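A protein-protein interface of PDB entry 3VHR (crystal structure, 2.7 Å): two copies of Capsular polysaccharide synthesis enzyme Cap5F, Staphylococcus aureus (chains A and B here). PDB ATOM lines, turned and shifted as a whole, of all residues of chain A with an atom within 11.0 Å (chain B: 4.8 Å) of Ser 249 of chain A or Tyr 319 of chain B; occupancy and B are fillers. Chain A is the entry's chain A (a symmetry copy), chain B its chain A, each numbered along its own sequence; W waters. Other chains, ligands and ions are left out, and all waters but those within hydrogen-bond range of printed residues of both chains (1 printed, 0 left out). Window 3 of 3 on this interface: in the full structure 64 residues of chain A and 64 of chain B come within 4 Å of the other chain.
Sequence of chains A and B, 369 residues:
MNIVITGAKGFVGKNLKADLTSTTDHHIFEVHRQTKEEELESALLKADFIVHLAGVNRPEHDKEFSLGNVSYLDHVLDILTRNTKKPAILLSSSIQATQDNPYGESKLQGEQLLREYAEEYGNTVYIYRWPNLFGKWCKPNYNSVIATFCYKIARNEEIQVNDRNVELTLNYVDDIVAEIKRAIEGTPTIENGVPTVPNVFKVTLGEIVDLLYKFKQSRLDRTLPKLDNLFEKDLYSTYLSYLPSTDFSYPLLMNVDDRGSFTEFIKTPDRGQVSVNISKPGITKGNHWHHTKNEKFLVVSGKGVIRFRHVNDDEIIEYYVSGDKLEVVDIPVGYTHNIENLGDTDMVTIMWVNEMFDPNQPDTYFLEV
Of the 12 printed residues of chain B, 6 touch a printed residue of chain A. Printed residues of chain A that touch a printed residue of chain B: Arg 219, Ser 245, Thr 246, Asp 247, Phe 248, Ser 249, Tyr 250, Leu 252 and Phe 265. Hydrophobic or aromatic side chains of chain A within 4 Å of the printed part of chain B: Phe 248, Tyr 250, Leu 252 and Phe 265. Among the printed residues, 16 pairs touch across the chains. Among the printed residues, Asp or Glu carboxylates within 4 Å of a Lys or Arg side-chain nitrogen of the other chain: Arg 219 of chain A with Asp 330 of chain B.
O of Phe 308 of chain B lies within hydrogen-bond range of N of Ile 317 of chain B, at 2.8 Å. NH1 of Arg 222 of chain A is in hydrogen-bond range of O of Arg 219 of chain A (2.8 Å). NH2 of Arg 219 of chain A lies within salt-bridge range of OD1 of Asp 247 of chain A, at 3.5 Å.
Printed residues of chain B within 4 Å of Ser 249 of chain A: Tyr 319 (3.2 Å), Val 328 (3.0 Å) and Val 329 (3.997 Å). Tyr 319 of chain B touches five residues of chain A. No residue of chain A comes within 4 Å of Ile 306 of chain B. No residue of chain A comes within 4 Å of Glu 318 of chain B. No residue of chain A comes within 4 Å of Val 321 of chain B. Asp 330 of chain B touches just these residues of chain A: Arg 219, Phe 248 and Tyr 250. Of the printed residues of chain B, Ser 245 of chain A touches Ile 317 (3.5 Å) and Tyr 319 (2.7 Å). Of the printed residues of chain A, Val 329 of chain B touches Phe 248 (3.7 Å) and Ser 249 (3.997 Å). The nearest printed residue of chain B that does not touch Ser 249 of chain A is Asp 330 of chain B (4.7 Å). The nearest residue of chain A that does not touch Tyr 319 of chain B is Pro 244 of chain A (4.9 Å).
Water W1 lies within hydrogen-bond range of OH of Tyr 236 of chain A and OD1 of Asp 330 of chain B.
N of Tyr 250 of chain A is in hydrogen-bond range of O of Val 328 of chain B, 3.0 Å away. The backbone carbonyl oxygen of Phe 248 of chain A is in hydrogen-bond range of the backbone NH of Asp 330 of chain B, at 2.8 Å. The side-chain hydroxyl (OH) of Tyr 319 of chain B lies within hydrogen-bond range of the backbone NH (N) of Asp 247 of chain A, 3.0 Å away. The guanidinium group (NH1) of Arg 219 of chain A lies within salt-bridge range of the side-chain carboxylate (OD2) of Asp 330 of chain B, at 2.5 Å. The backbone NH (N) of Phe 248 of chain A sits at hydrogen-bond distance from the side-chain hydroxyl (OH) of Tyr 319 of chain B, at 2.9 Å. OH of Tyr 319 of chain B lies within hydrogen-bond range of O of Ser 245 of chain A, 2.7 Å away. OH of Tyr 319 of chain B sits close to O of Thr 246 of chain A, 3.2 Å away.
Among the printed residues, pairs that only touch across the chains: Ser 249 of chain A with Val 328 of chain B (3.0 Å), Ser 249 of chain A with Tyr 319 of chain B (3.2 Å), Tyr 250 of chain A with Asp 330 of chain B (3.4 Å), Ser 245 of chain A with Ile 317 of chain B (3.5 Å), Leu 252 of chain A with Val 328 of chain B (3.5 Å), Phe 265 of chain A with Val 328 of chain B (3.6 Å), Phe 248 of chain A with Phe 308 of chain B (3.7 Å), Phe 248 of chain A with Val 329 of chain B (3.7 Å) and Ser 249 of chain A with Val 329 of chain B (3.997 Å).
No position is printed for both chains. Of the 16 pairs that touch across the chains among the printed residues, none has its exchanged pair printed and touching as well.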
ATOM      1  N   ALA A 154      -4.871  10.916  14.280  1.00  0.00           N
ATOM      2  CA  ALA A 154      -4.828  11.135  12.845  1.00  0.00           C
ATOM      3  C   ALA A 154      -3.417  10.952  12.353  1.00  0.00           C
ATOM      4  O   ALA A 154      -3.199  10.733  11.159  1.00  0.00           O
ATOM      5  CB  ALA A 154      -5.321  12.528  12.508  1.00  0.00           C
ATOM      6  N   LYS A 216     -10.978   6.740  12.092  1.00  0.00           N
ATOM      7  CA  LYS A 216      -9.734   6.431  11.404  1.00  0.00           C
ATOM      8  C   LYS A 216      -9.780   5.078  10.713  1.00  0.00           C
ATOM      9  O   LYS A 216      -9.207   4.920   9.636  1.00  0.00           O
ATOM     10  CB  LYS A 216      -8.548   6.463  12.359  1.00  0.00           C
ATOM     11  CG  LYS A 216      -7.247   6.676  11.624  1.00  0.00           C
ATOM     12  CD  LYS A 216      -6.068   6.325  12.487  1.00  0.00           C
ATOM     13  CE  LYS A 216      -4.803   6.453  11.668  1.00  0.00           C
ATOM     14  NZ  LYS A 216      -3.884   5.345  12.048  1.00  0.00           N
ATOM     15  N   SER A 218     -12.317   3.806   9.391  1.00  0.00           N
ATOM     16  CA  SER A 218     -13.286   3.871   8.314  1.00  0.00           C
ATOM     17  C   SER A 218     -12.678   4.177   6.960  1.00  0.00           C
ATOM     18  O   SER A 218     -13.333   3.979   5.939  1.00  0.00           O
ATOM     19  CB  SER A 218     -14.375   4.883   8.636  1.00  0.00           C
ATOM     20  OG  SER A 218     -15.280   4.333   9.570  1.00  0.00           O
ATOM     21  N   ARG A 219     -11.442   4.662   6.944  1.00  0.00           N
ATOM     22  CA  ARG A 219     -10.705   4.783   5.694  1.00  0.00           C
ATOM     23  C   ARG A 219     -10.398   3.387   5.163  1.00  0.00           C
ATOM     24  O   ARG A 219     -10.319   3.187   3.955  1.00  0.00           O
ATOM     25  CB  ARG A 219      -9.398   5.564   5.871  1.00  0.00           C
ATOM     26  CG  ARG A 219      -9.501   6.794   6.752  1.00  0.00           C
ATOM     27  CD  ARG A 219      -9.583   8.073   5.959  1.00  0.00           C
ATOM     28  NE  ARG A 219      -8.255   8.648   5.751  1.00  0.00           N
ATOM     29  CZ  ARG A 219      -8.019   9.916   5.414  1.00  0.00           C
ATOM     30  NH1 ARG A 219      -8.999  10.792   5.237  1.00  0.00           N
ATOM     31  NH2 ARG A 219      -6.780  10.308   5.255  1.00  0.00           N
ATOM     32  N   LEU A 220     -10.240   2.419   6.060  1.00  0.00           N
ATOM     33  CA  LEU A 220      -9.891   1.059   5.659  1.00  0.00           C
ATOM     34  C   LEU A 220     -11.107   0.197   5.316  1.00  0.00           C
ATOM     35  O   LEU A 220     -11.061  -0.599   4.378  1.00  0.00           O
ATOM     36  CB  LEU A 220      -9.017   0.382   6.721  1.00  0.00           C
ATOM     37  CG  LEU A 220      -7.484   0.578   6.708  1.00  0.00           C
ATOM     38  CD1 LEU A 220      -7.023   1.825   5.969  1.00  0.00           C
ATOM     39  CD2 LEU A 220      -6.919   0.575   8.124  1.00  0.00           C
ATOM     40  N   ARG A 222     -14.366   1.414   4.725  1.00  0.00           N
ATOM     41  CA  ARG A 222     -15.341   2.181   3.925  1.00  0.00           C
ATOM     42  C   ARG A 222     -16.674   2.419   4.637  1.00  0.00           C
ATOM     43  O   ARG A 222     -17.671   2.746   3.996  1.00  0.00           O
ATOM     44  CB  ARG A 222     -15.630   1.531   2.557  1.00  0.00           C
ATOM     45  CG  ARG A 222     -14.547   0.664   1.958  1.00  0.00           C
ATOM     46  CD  ARG A 222     -13.401   1.490   1.438  1.00  0.00           C
ATOM     47  NE  ARG A 222     -12.359   0.611   0.923  1.00  0.00           N
ATOM     48  CZ  ARG A 222     -11.065   0.910   0.923  1.00  0.00           C
ATOM     49  NH1 ARG A 222     -10.639   2.067   1.423  1.00  0.00           N
ATOM     50  NH2 ARG A 222     -10.193   0.047   0.430  1.00  0.00           N
ATOM     51  N   TYR A 236     -17.124  13.968  14.426  1.00  0.00           N
ATOM     52  CA  TYR A 236     -16.549  13.546  13.150  1.00  0.00           C
ATOM     53  C   TYR A 236     -16.029  14.744  12.372  1.00  0.00           C
ATOM     54  O   TYR A 236     -14.909  14.726  11.849  1.00  0.00           O
ATOM     55  CB  TYR A 236     -17.560  12.731  12.317  1.00  0.00           C
ATOM     56  CG  TYR A 236     -17.016  12.252  10.978  1.00  0.00           C
ATOM     57  CD1 TYR A 236     -15.987  11.319  10.918  1.00  0.00           C
ATOM     58  CD2 TYR A 236     -17.530  12.732   9.771  1.00  0.00           C
ATOM     59  CE1 TYR A 236     -15.482  10.879   9.699  1.00  0.00           C
ATOM     60  CE2 TYR A 236     -17.026  12.301   8.549  1.00  0.00           C
ATOM     61  CZ  TYR A 236     -16.006  11.374   8.524  1.00  0.00           C
ATOM     62  OH  TYR A 236     -15.486  10.923   7.340  1.00  0.00           O
ATOM     63  N   TYR A 239     -12.872  16.013  14.124  1.00  0.00           N
ATOM     64  CA  TYR A 239     -11.728  15.127  13.867  1.00  0.00           C
ATOM     65  C   TYR A 239     -11.103  15.385  12.495  1.00  0.00           C
ATOM     66  O   TYR A 239      -9.879  15.448  12.367  1.00  0.00           O
ATOM     67  CB  TYR A 239     -12.091  13.636  14.048  1.00  0.00           C
ATOM     68  CG  TYR A 239     -11.014  12.686  13.577  1.00  0.00           C
ATOM     69  CD1 TYR A 239      -9.868  12.447  14.339  1.00  0.00           C
ATOM     70  CD2 TYR A 239     -11.128  12.042  12.348  1.00  0.00           C
ATOM     71  CE1 TYR A 239      -8.869  11.580  13.883  1.00  0.00           C
ATOM     72  CE2 TYR A 239     -10.153  11.174  11.884  1.00  0.00           C
ATOM     73  CZ  TYR A 239      -9.031  10.943  12.648  1.00  0.00           C
ATOM     74  OH  TYR A 239      -8.087  10.088  12.154  1.00  0.00           O
ATOM     75  N   LEU A 240     -11.945  15.545  11.480  1.00  0.00           N
ATOM     76  CA  LEU A 240     -11.461  15.768  10.130  1.00  0.00           C
ATOM     77  C   LEU A 240     -10.587  16.997  10.083  1.00  0.00           C
ATOM     78  O   LEU A 240      -9.561  16.992   9.416  1.00  0.00           O
ATOM     79  CB  LEU A 240     -12.621  15.911   9.152  1.00  0.00           C
ATOM     80  CG  LEU A 240     -13.034  14.762   8.229  1.00  0.00           C
ATOM     81  CD1 LEU A 240     -12.714  13.368   8.749  1.00  0.00           C
ATOM     82  CD2 LEU A 240     -14.513  14.926   7.918  1.00  0.00           C
ATOM     83  N   TYR A 242      -8.450  18.101  11.964  1.00  0.00           N
ATOM     84  CA  TYR A 242      -7.086  17.867  12.484  1.00  0.00           C
ATOM     85  C   TYR A 242      -6.183  17.009  11.602  1.00  0.00           C
ATOM     86  O   TYR A 242      -5.026  16.743  11.960  1.00  0.00           O
ATOM     87  CB  TYR A 242      -7.141  17.273  13.894  1.00  0.00           C
ATOM     88  CG  TYR A 242      -7.615  18.273  14.906  1.00  0.00           C
ATOM     89  CD1 TYR A 242      -6.744  19.221  15.442  1.00  0.00           C
ATOM     90  CD2 TYR A 242      -8.943  18.302  15.301  1.00  0.00           C
ATOM     91  CE1 TYR A 242      -7.188  20.161  16.361  1.00  0.00           C
ATOM     92  CE2 TYR A 242      -9.399  19.230  16.217  1.00  0.00           C
ATOM     93  CZ  TYR A 242      -8.524  20.162  16.739  1.00  0.00           C
ATOM     94  OH  TYR A 242      -8.991  21.080  17.644  1.00  0.00           O
ATOM     95  N   LEU A 243      -6.703  16.571  10.461  1.00  0.00           N
ATOM     96  CA  LEU A 243      -5.935  15.780   9.504  1.00  0.00           C
ATOM     97  C   LEU A 243      -4.735  16.564   8.970  1.00  0.00           C
ATOM     98  O   LEU A 243      -4.871  17.740   8.663  1.00  0.00           O
ATOM     99  CB  LEU A 243      -6.842  15.385   8.337  1.00  0.00           C
ATOM    100  CG  LEU A 243      -7.402  13.979   8.087  1.00  0.00           C
ATOM    101  CD1 LEU A 243      -7.452  13.073   9.300  1.00  0.00           C
ATOM    102  CD2 LEU A 243      -8.779  14.114   7.463  1.00  0.00           C
ATOM    103  N   PRO A 244      -3.551  15.925   8.854  1.00  0.00           N
ATOM    104  CA  PRO A 244      -2.477  16.635   8.156  1.00  0.00           C
ATOM    105  C   PRO A 244      -2.919  17.007   6.738  1.00  0.00           C
ATOM    106  O   PRO A 244      -3.657  16.253   6.107  1.00  0.00           O
ATOM    107  CB  PRO A 244      -1.344  15.602   8.105  1.00  0.00           C
ATOM    108  CG  PRO A 244      -1.628  14.665   9.226  1.00  0.00           C
ATOM    109  CD  PRO A 244      -3.129  14.575   9.278  1.00  0.00           C
ATOM    110  N   SER A 245      -2.488  18.168   6.253  1.00  0.00           N
ATOM    111  CA  SER A 245      -2.870  18.659   4.916  1.00  0.00           C
ATOM    112  C   SER A 245      -2.459  17.745   3.743  1.00  0.00           C
ATOM    113  O   SER A 245      -3.021  17.844   2.647  1.00  0.00           O
ATOM    114  CB  SER A 245      -2.316  20.066   4.696  1.00  0.00           C
ATOM    115  OG  SER A 245      -0.912  20.023   4.561  1.00  0.00           O
ATOM    116  N   THR A 246      -1.480  16.871   3.971  1.00  0.00           N
ATOM    117  CA  THR A 246      -1.028  15.919   2.954  1.00  0.00           C
ATOM    118  C   THR A 246      -1.864  14.643   2.971  1.00  0.00           C
ATOM    119  O   THR A 246      -1.641  13.730   2.194  1.00  0.00           O
ATOM    120  CB  THR A 246       0.435  15.517   3.199  1.00  0.00           C
ATOM    121  OG1 THR A 246       0.581  15.074   4.553  1.00  0.00           O
ATOM    122  CG2 THR A 246       1.368  16.694   2.946  1.00  0.00           C
ATOM    123  N   ASP A 247      -2.855  14.611   3.846  1.00  0.00           N
ATOM    124  CA  ASP A 247      -3.480  13.374   4.256  1.00  0.00           C
ATOM    125  C   ASP A 247      -5.004  13.355   4.094  1.00  0.00           C
ATOM    126  O   ASP A 247      -5.683  12.632   4.803  1.00  0.00           O
ATOM    127  CB  ASP A 247      -3.117  13.137   5.717  1.00  0.00           C
ATOM    128  CG  ASP A 247      -2.750  11.711   5.997  1.00  0.00           C
ATOM    129  OD1 ASP A 247      -3.329  10.802   5.347  1.00  0.00           O
ATOM    130  OD2 ASP A 247      -1.875  11.505   6.871  1.00  0.00           O
ATOM    131  N   PHE A 248      -5.531  14.133   3.156  1.00  0.00           N
ATOM    132  CA  PHE A 248      -6.972  14.255   2.980  1.00  0.00           C
ATOM    133  C   PHE A 248      -7.594  13.100   2.198  1.00  0.00           C
ATOM    134  O   PHE A 248      -8.817  12.903   2.235  1.00  0.00           O
ATOM    135  CB  PHE A 248      -7.323  15.565   2.270  1.00  0.00           C
ATOM    136  CG  PHE A 248      -7.087  16.803   3.091  1.00  0.00           C
ATOM    137  CD1 PHE A 248      -6.619  16.730   4.401  1.00  0.00           C
ATOM    138  CD2 PHE A 248      -7.374  18.056   2.561  1.00  0.00           C
ATOM    139  CE1 PHE A 248      -6.410  17.882   5.149  1.00  0.00           C
ATOM    140  CE2 PHE A 248      -7.176  19.206   3.311  1.00  0.00           C
ATOM    141  CZ  PHE A 248      -6.690  19.117   4.602  1.00  0.00           C
ATOM    142  N   SER A 249      -6.768  12.360   1.467  1.00  0.00           N
ATOM    143  CA  SER A 249      -7.276  11.330   0.579  1.00  0.00           C
ATOM    144  C   SER A 249      -6.754   9.956   0.966  1.00  0.00           C
ATOM    145  O   SER A 249      -5.703   9.830   1.615  1.00  0.00           O
ATOM    146  CB  SER A 249      -6.933  11.656  -0.881  1.00  0.00           C
ATOM    147  OG  SER A 249      -5.539  11.740  -1.067  1.00  0.00           O
ATOM    148  N   TYR A 250      -7.497   8.929   0.573  1.00  0.00           N
ATOM    149  CA  TYR A 250      -7.109   7.562   0.870  1.00  0.00           C
ATOM    150  C   TYR A 250      -7.421   6.689  -0.314  1.00  0.00           C
ATOM    151  O   TYR A 250      -8.414   6.909  -0.986  1.00  0.00           O
ATOM    152  CB  TYR A 250      -7.798   7.041   2.139  1.00  0.00           C
ATOM    153  CG  TYR A 250      -9.305   7.230   2.208  1.00  0.00           C
ATOM    154  CD1 TYR A 250      -9.859   8.470   2.542  1.00  0.00           C
ATOM    155  CD2 TYR A 250     -10.172   6.158   1.978  1.00  0.00           C
ATOM    156  CE1 TYR A 250     -11.222   8.641   2.636  1.00  0.00           C
ATOM    157  CE2 TYR A 250     -11.541   6.317   2.067  1.00  0.00           C
ATOM    158  CZ  TYR A 250     -12.064   7.562   2.399  1.00  0.00           C
ATOM    159  OH  TYR A 250     -13.441   7.740   2.479  1.00  0.00           O
ATOM    160  N   PRO A 251      -6.555   5.707  -0.596  1.00  0.00           N
ATOM    161  CA  PRO A 251      -6.812   4.881  -1.770  1.00  0.00           C
ATOM    162  C   PRO A 251      -7.972   3.927  -1.547  1.00  0.00           C
ATOM    163  O   PRO A 251      -8.247   3.517  -0.414  1.00  0.00           O
ATOM    164  CB  PRO A 251      -5.511   4.106  -1.949  1.00  0.00           C
ATOM    165  CG  PRO A 251      -4.920   4.052  -0.577  1.00  0.00           C
ATOM    166  CD  PRO A 251      -5.291   5.351   0.074  1.00  0.00           C
ATOM    167  N   LEU A 252      -8.665   3.622  -2.633  1.00  0.00           N
ATOM    168  CA  LEU A 252      -9.712   2.617  -2.659  1.00  0.00           C
ATOM    169  C   LEU A 252      -9.146   1.358  -3.308  1.00  0.00           C
ATOM    170  O   LEU A 252      -8.219   1.447  -4.104  1.00  0.00           O
ATOM    171  CB  LEU A 252     -10.877   3.137  -3.494  1.00  0.00           C
ATOM    172  CG  LEU A 252     -12.214   3.513  -2.867  1.00  0.00           C
ATOM    173  CD1 LEU A 252     -12.102   4.126  -1.488  1.00  0.00           C
ATOM    174  CD2 LEU A 252     -12.964   4.429  -3.816  1.00  0.00           C
ATOM    175  N   LEU A 253      -9.698   0.192  -2.973  1.00  0.00           N
ATOM    176  CA  LEU A 253      -9.276  -1.065  -3.596  1.00  0.00           C
ATOM    177  C   LEU A 253     -10.055  -1.332  -4.886  1.00  0.00           C
ATOM    178  O   LEU A 253     -11.218  -1.753  -4.845  1.00  0.00           O
ATOM    179  CB  LEU A 253      -9.385  -2.263  -2.633  1.00  0.00           C
ATOM    180  CG  LEU A 253      -8.654  -3.528  -3.162  1.00  0.00           C
ATOM    181  CD1 LEU A 253      -7.201  -3.615  -2.693  1.00  0.00           C
ATOM    182  CD2 LEU A 253      -9.398  -4.837  -2.879  1.00  0.00           C
ATOM    183  N   PHE A 265     -16.847   1.796  -2.365  1.00  0.00           N
ATOM    184  CA  PHE A 265     -16.665   3.202  -1.979  1.00  0.00           C
ATOM    185  C   PHE A 265     -17.120   3.451  -0.527  1.00  0.00           C
ATOM    186  O   PHE A 265     -16.290   3.772   0.341  1.00  0.00           O
ATOM    187  CB  PHE A 265     -17.405   4.100  -2.978  1.00  0.00           C
ATOM    188  CG  PHE A 265     -17.541   5.540  -2.555  1.00  0.00           C
ATOM    189  CD1 PHE A 265     -16.512   6.207  -1.877  1.00  0.00           C
ATOM    190  CD2 PHE A 265     -18.693   6.263  -2.879  1.00  0.00           C
ATOM    191  CE1 PHE A 265     -16.649   7.546  -1.505  1.00  0.00           C
ATOM    192  CE2 PHE A 265     -18.820   7.607  -2.510  1.00  0.00           C
ATOM    193  CZ  PHE A 265     -17.795   8.249  -1.826  1.00  0.00           C
ATOM    194  N   GLY B 304      -8.730  15.911 -13.023  1.00  0.00           N
ATOM    195  CA  GLY B 304      -8.624  17.290 -12.562  1.00  0.00           C
ATOM    196  C   GLY B 304      -7.958  17.448 -11.219  1.00  0.00           C
ATOM    197  O   GLY B 304      -7.182  16.586 -10.793  1.00  0.00           O
ATOM    198  N   VAL B 305      -8.265  18.558 -10.553  1.00  0.00           N
ATOM    199  CA  VAL B 305      -7.651  18.881  -9.264  1.00  0.00           C
ATOM    200  C   VAL B 305      -8.685  19.359  -8.228  1.00  0.00           C
ATOM    201  O   VAL B 305      -9.583  20.148  -8.558  1.00  0.00           O
ATOM    202  CB  VAL B 305      -6.498  19.901  -9.431  1.00  0.00           C
ATOM    203  CG1 VAL B 305      -7.019  21.238  -9.936  1.00  0.00           C
ATOM    204  CG2 VAL B 305      -5.718  20.063  -8.134  1.00  0.00           C
ATOM    205  N   ILE B 306      -8.575  18.842  -6.998  1.00  0.00           N
ATOM    206  CA  ILE B 306      -9.343  19.344  -5.846  1.00  0.00           C
ATOM    207  C   ILE B 306      -8.398  20.182  -4.981  1.00  0.00           C
ATOM    208  O   ILE B 306      -7.371  19.673  -4.532  1.00  0.00           O
ATOM    209  CB  ILE B 306      -9.959  18.207  -5.004  1.00  0.00           C
ATOM    210  CG1 ILE B 306     -10.932  17.377  -5.834  1.00  0.00           C
ATOM    211  CG2 ILE B 306     -10.717  18.785  -3.829  1.00  0.00           C
ATOM    212  CD1 ILE B 306     -11.079  15.940  -5.381  1.00  0.00           C
ATOM    213  N   PHE B 308      -7.526  23.012  -1.694  1.00  0.00           N
ATOM    214  CA  PHE B 308      -7.875  23.398  -0.324  1.00  0.00           C
ATOM    215  C   PHE B 308      -7.019  24.557   0.196  1.00  0.00           C
ATOM    216  O   PHE B 308      -5.796  24.569   0.025  1.00  0.00           O
ATOM    217  CB  PHE B 308      -7.664  22.234   0.640  1.00  0.00           C
ATOM    218  CG  PHE B 308      -8.379  20.973   0.264  1.00  0.00           C
ATOM    219  CD1 PHE B 308      -9.631  20.696   0.782  1.00  0.00           C
ATOM    220  CD2 PHE B 308      -7.778  20.035  -0.565  1.00  0.00           C
ATOM    221  CE1 PHE B 308     -10.284  19.517   0.456  1.00  0.00           C
ATOM    222  CE2 PHE B 308      -8.420  18.855  -0.895  1.00  0.00           C
ATOM    223  CZ  PHE B 308      -9.675  18.594  -0.385  1.00  0.00           C
ATOM    224  N   ILE B 317      -3.331  23.787  -1.086  1.00  0.00           N
ATOM    225  CA  ILE B 317      -2.952  22.383  -1.212  1.00  0.00           C
ATOM    226  C   ILE B 317      -3.740  21.755  -2.356  1.00  0.00           C
ATOM    227  O   ILE B 317      -4.978  21.812  -2.385  1.00  0.00           O
ATOM    228  CB  ILE B 317      -3.224  21.611   0.101  1.00  0.00           C
ATOM    229  CG1 ILE B 317      -2.576  22.334   1.284  1.00  0.00           C
ATOM    230  CG2 ILE B 317      -2.698  20.185   0.020  1.00  0.00           C
ATOM    231  CD1 ILE B 317      -3.538  22.675   2.398  1.00  0.00           C
ATOM    232  N   GLU B 318      -3.024  21.155  -3.304  1.00  0.00           N
ATOM    233  CA  GLU B 318      -3.665  20.567  -4.480  1.00  0.00           C
ATOM    234  C   GLU B 318      -3.688  19.031  -4.451  1.00  0.00           C
ATOM    235  O   GLU B 318      -2.686  18.402  -4.126  1.00  0.00           O
ATOM    236  CB  GLU B 318      -2.992  21.096  -5.747  1.00  0.00           C
ATOM    237  CG  GLU B 318      -3.065  22.610  -5.889  1.00  0.00           C
ATOM    238  CD  GLU B 318      -2.586  23.099  -7.251  1.00  0.00           C
ATOM    239  OE1 GLU B 318      -1.479  22.699  -7.677  1.00  0.00           O
ATOM    240  OE2 GLU B 318      -3.311  23.890  -7.903  1.00  0.00           O
ATOM    241  N   TYR B 319      -4.840  18.440  -4.776  1.00  0.00           N
ATOM    242  CA  TYR B 319      -4.961  16.978  -4.961  1.00  0.00           C
ATOM    243  C   TYR B 319      -5.311  16.618  -6.408  1.00  0.00           C
ATOM    244  O   TYR B 319      -6.467  16.743  -6.829  1.00  0.00           O
ATOM    245  CB  TYR B 319      -5.992  16.362  -3.994  1.00  0.00           C
ATOM    246  CG  TYR B 319      -5.461  16.164  -2.596  1.00  0.00           C
ATOM    247  CD1 TYR B 319      -4.938  14.937  -2.194  1.00  0.00           C
ATOM    248  CD2 TYR B 319      -5.463  17.213  -1.681  1.00  0.00           C
ATOM    249  CE1 TYR B 319      -4.426  14.764  -0.917  1.00  0.00           C
ATOM    250  CE2 TYR B 319      -4.957  17.053  -0.406  1.00  0.00           C
ATOM    251  CZ  TYR B 319      -4.443  15.833  -0.027  1.00  0.00           C
ATOM    252  OH  TYR B 319      -3.948  15.688   1.243  1.00  0.00           O
ATOM    253  N   TYR B 320      -4.317  16.168  -7.167  1.00  0.00           N
ATOM    254  CA  TYR B 320      -4.559  15.758  -8.543  1.00  0.00           C
ATOM    255  C   TYR B 320      -5.167  14.376  -8.569  1.00  0.00           C
ATOM    256  O   TYR B 320      -4.620  13.441  -7.998  1.00  0.00           O
ATOM    257  CB  TYR B 320      -3.279  15.843  -9.379  1.00  0.00           C
ATOM    258  CG  TYR B 320      -2.874  17.272  -9.600  1.00  0.00           C
ATOM    259  CD1 TYR B 320      -2.023  17.912  -8.706  1.00  0.00           C
ATOM    260  CD2 TYR B 320      -3.385  18.002 -10.667  1.00  0.00           C
ATOM    261  CE1 TYR B 320      -1.663  19.234  -8.886  1.00  0.00           C
ATOM    262  CE2 TYR B 320      -3.036  19.327 -10.855  1.00  0.00           C
ATOM    263  CZ  TYR B 320      -2.173  19.934  -9.962  1.00  0.00           C
ATOM    264  OH  TYR B 320      -1.811  21.246 -10.129  1.00  0.00           O
ATOM    265  N   VAL B 321      -6.320  14.268  -9.214  1.00  0.00           N
ATOM    266  CA  VAL B 321      -7.116  13.039  -9.193  1.00  0.00           C
ATOM    267  C   VAL B 321      -7.715  12.779 -10.559  1.00  0.00           C
ATOM    268  O   VAL B 321      -7.939  13.717 -11.346  1.00  0.00           O
ATOM    269  CB  VAL B 321      -8.274  13.089  -8.147  1.00  0.00           C
ATOM    270  CG1 VAL B 321      -7.748  12.927  -6.729  1.00  0.00           C
ATOM    271  CG2 VAL B 321      -9.084  14.376  -8.270  1.00  0.00           C
ATOM    272  N   VAL B 328     -10.690   8.498  -2.698  1.00  0.00           N
ATOM    273  CA  VAL B 328     -11.577   9.445  -2.036  1.00  0.00           C
ATOM    274  C   VAL B 328     -10.771  10.616  -1.482  1.00  0.00           C
ATOM    275  O   VAL B 328      -9.727  10.420  -0.871  1.00  0.00           O
ATOM    276  CB  VAL B 328     -12.335   8.777  -0.870  1.00  0.00           C
ATOM    277  CG1 VAL B 328     -13.303   9.753  -0.239  1.00  0.00           C
ATOM    278  CG2 VAL B 328     -13.060   7.525  -1.326  1.00  0.00           C
ATOM    279  N   VAL B 329     -11.253  11.832  -1.704  1.00  0.00           N
ATOM    280  CA  VAL B 329     -10.708  12.992  -1.019  1.00  0.00           C
ATOM    281  C   VAL B 329     -11.746  13.476   0.000  1.00  0.00           C
ATOM    282  O   VAL B 329     -12.838  13.879  -0.374  1.00  0.00           O
ATOM    283  CB  VAL B 329     -10.311  14.134  -1.982  1.00  0.00           C
ATOM    284  CG1 VAL B 329      -9.447  15.144  -1.253  1.00  0.00           C
ATOM    285  CG2 VAL B 329      -9.541  13.619  -3.188  1.00  0.00           C
ATOM    286  N   ASP B 330     -11.414  13.378   1.291  1.00  0.00           N
ATOM    287  CA  ASP B 330     -12.216  13.983   2.355  1.00  0.00           C
ATOM    288  C   ASP B 330     -12.097  15.494   2.265  1.00  0.00           C
ATOM    289  O   ASP B 330     -11.029  16.029   1.992  1.00  0.00           O
ATOM    290  CB  ASP B 330     -11.734  13.525   3.729  1.00  0.00           C
ATOM    291  CG  ASP B 330     -12.172  12.130   4.059  1.00  0.00           C
ATOM    292  OD1 ASP B 330     -13.349  11.807   3.787  1.00  0.00           O
ATOM    293  OD2 ASP B 330     -11.347  11.358   4.609  1.00  0.00           O
HETATM  294  O   HOH W   1     -15.758  12.424   5.186  1.00  0.00           O
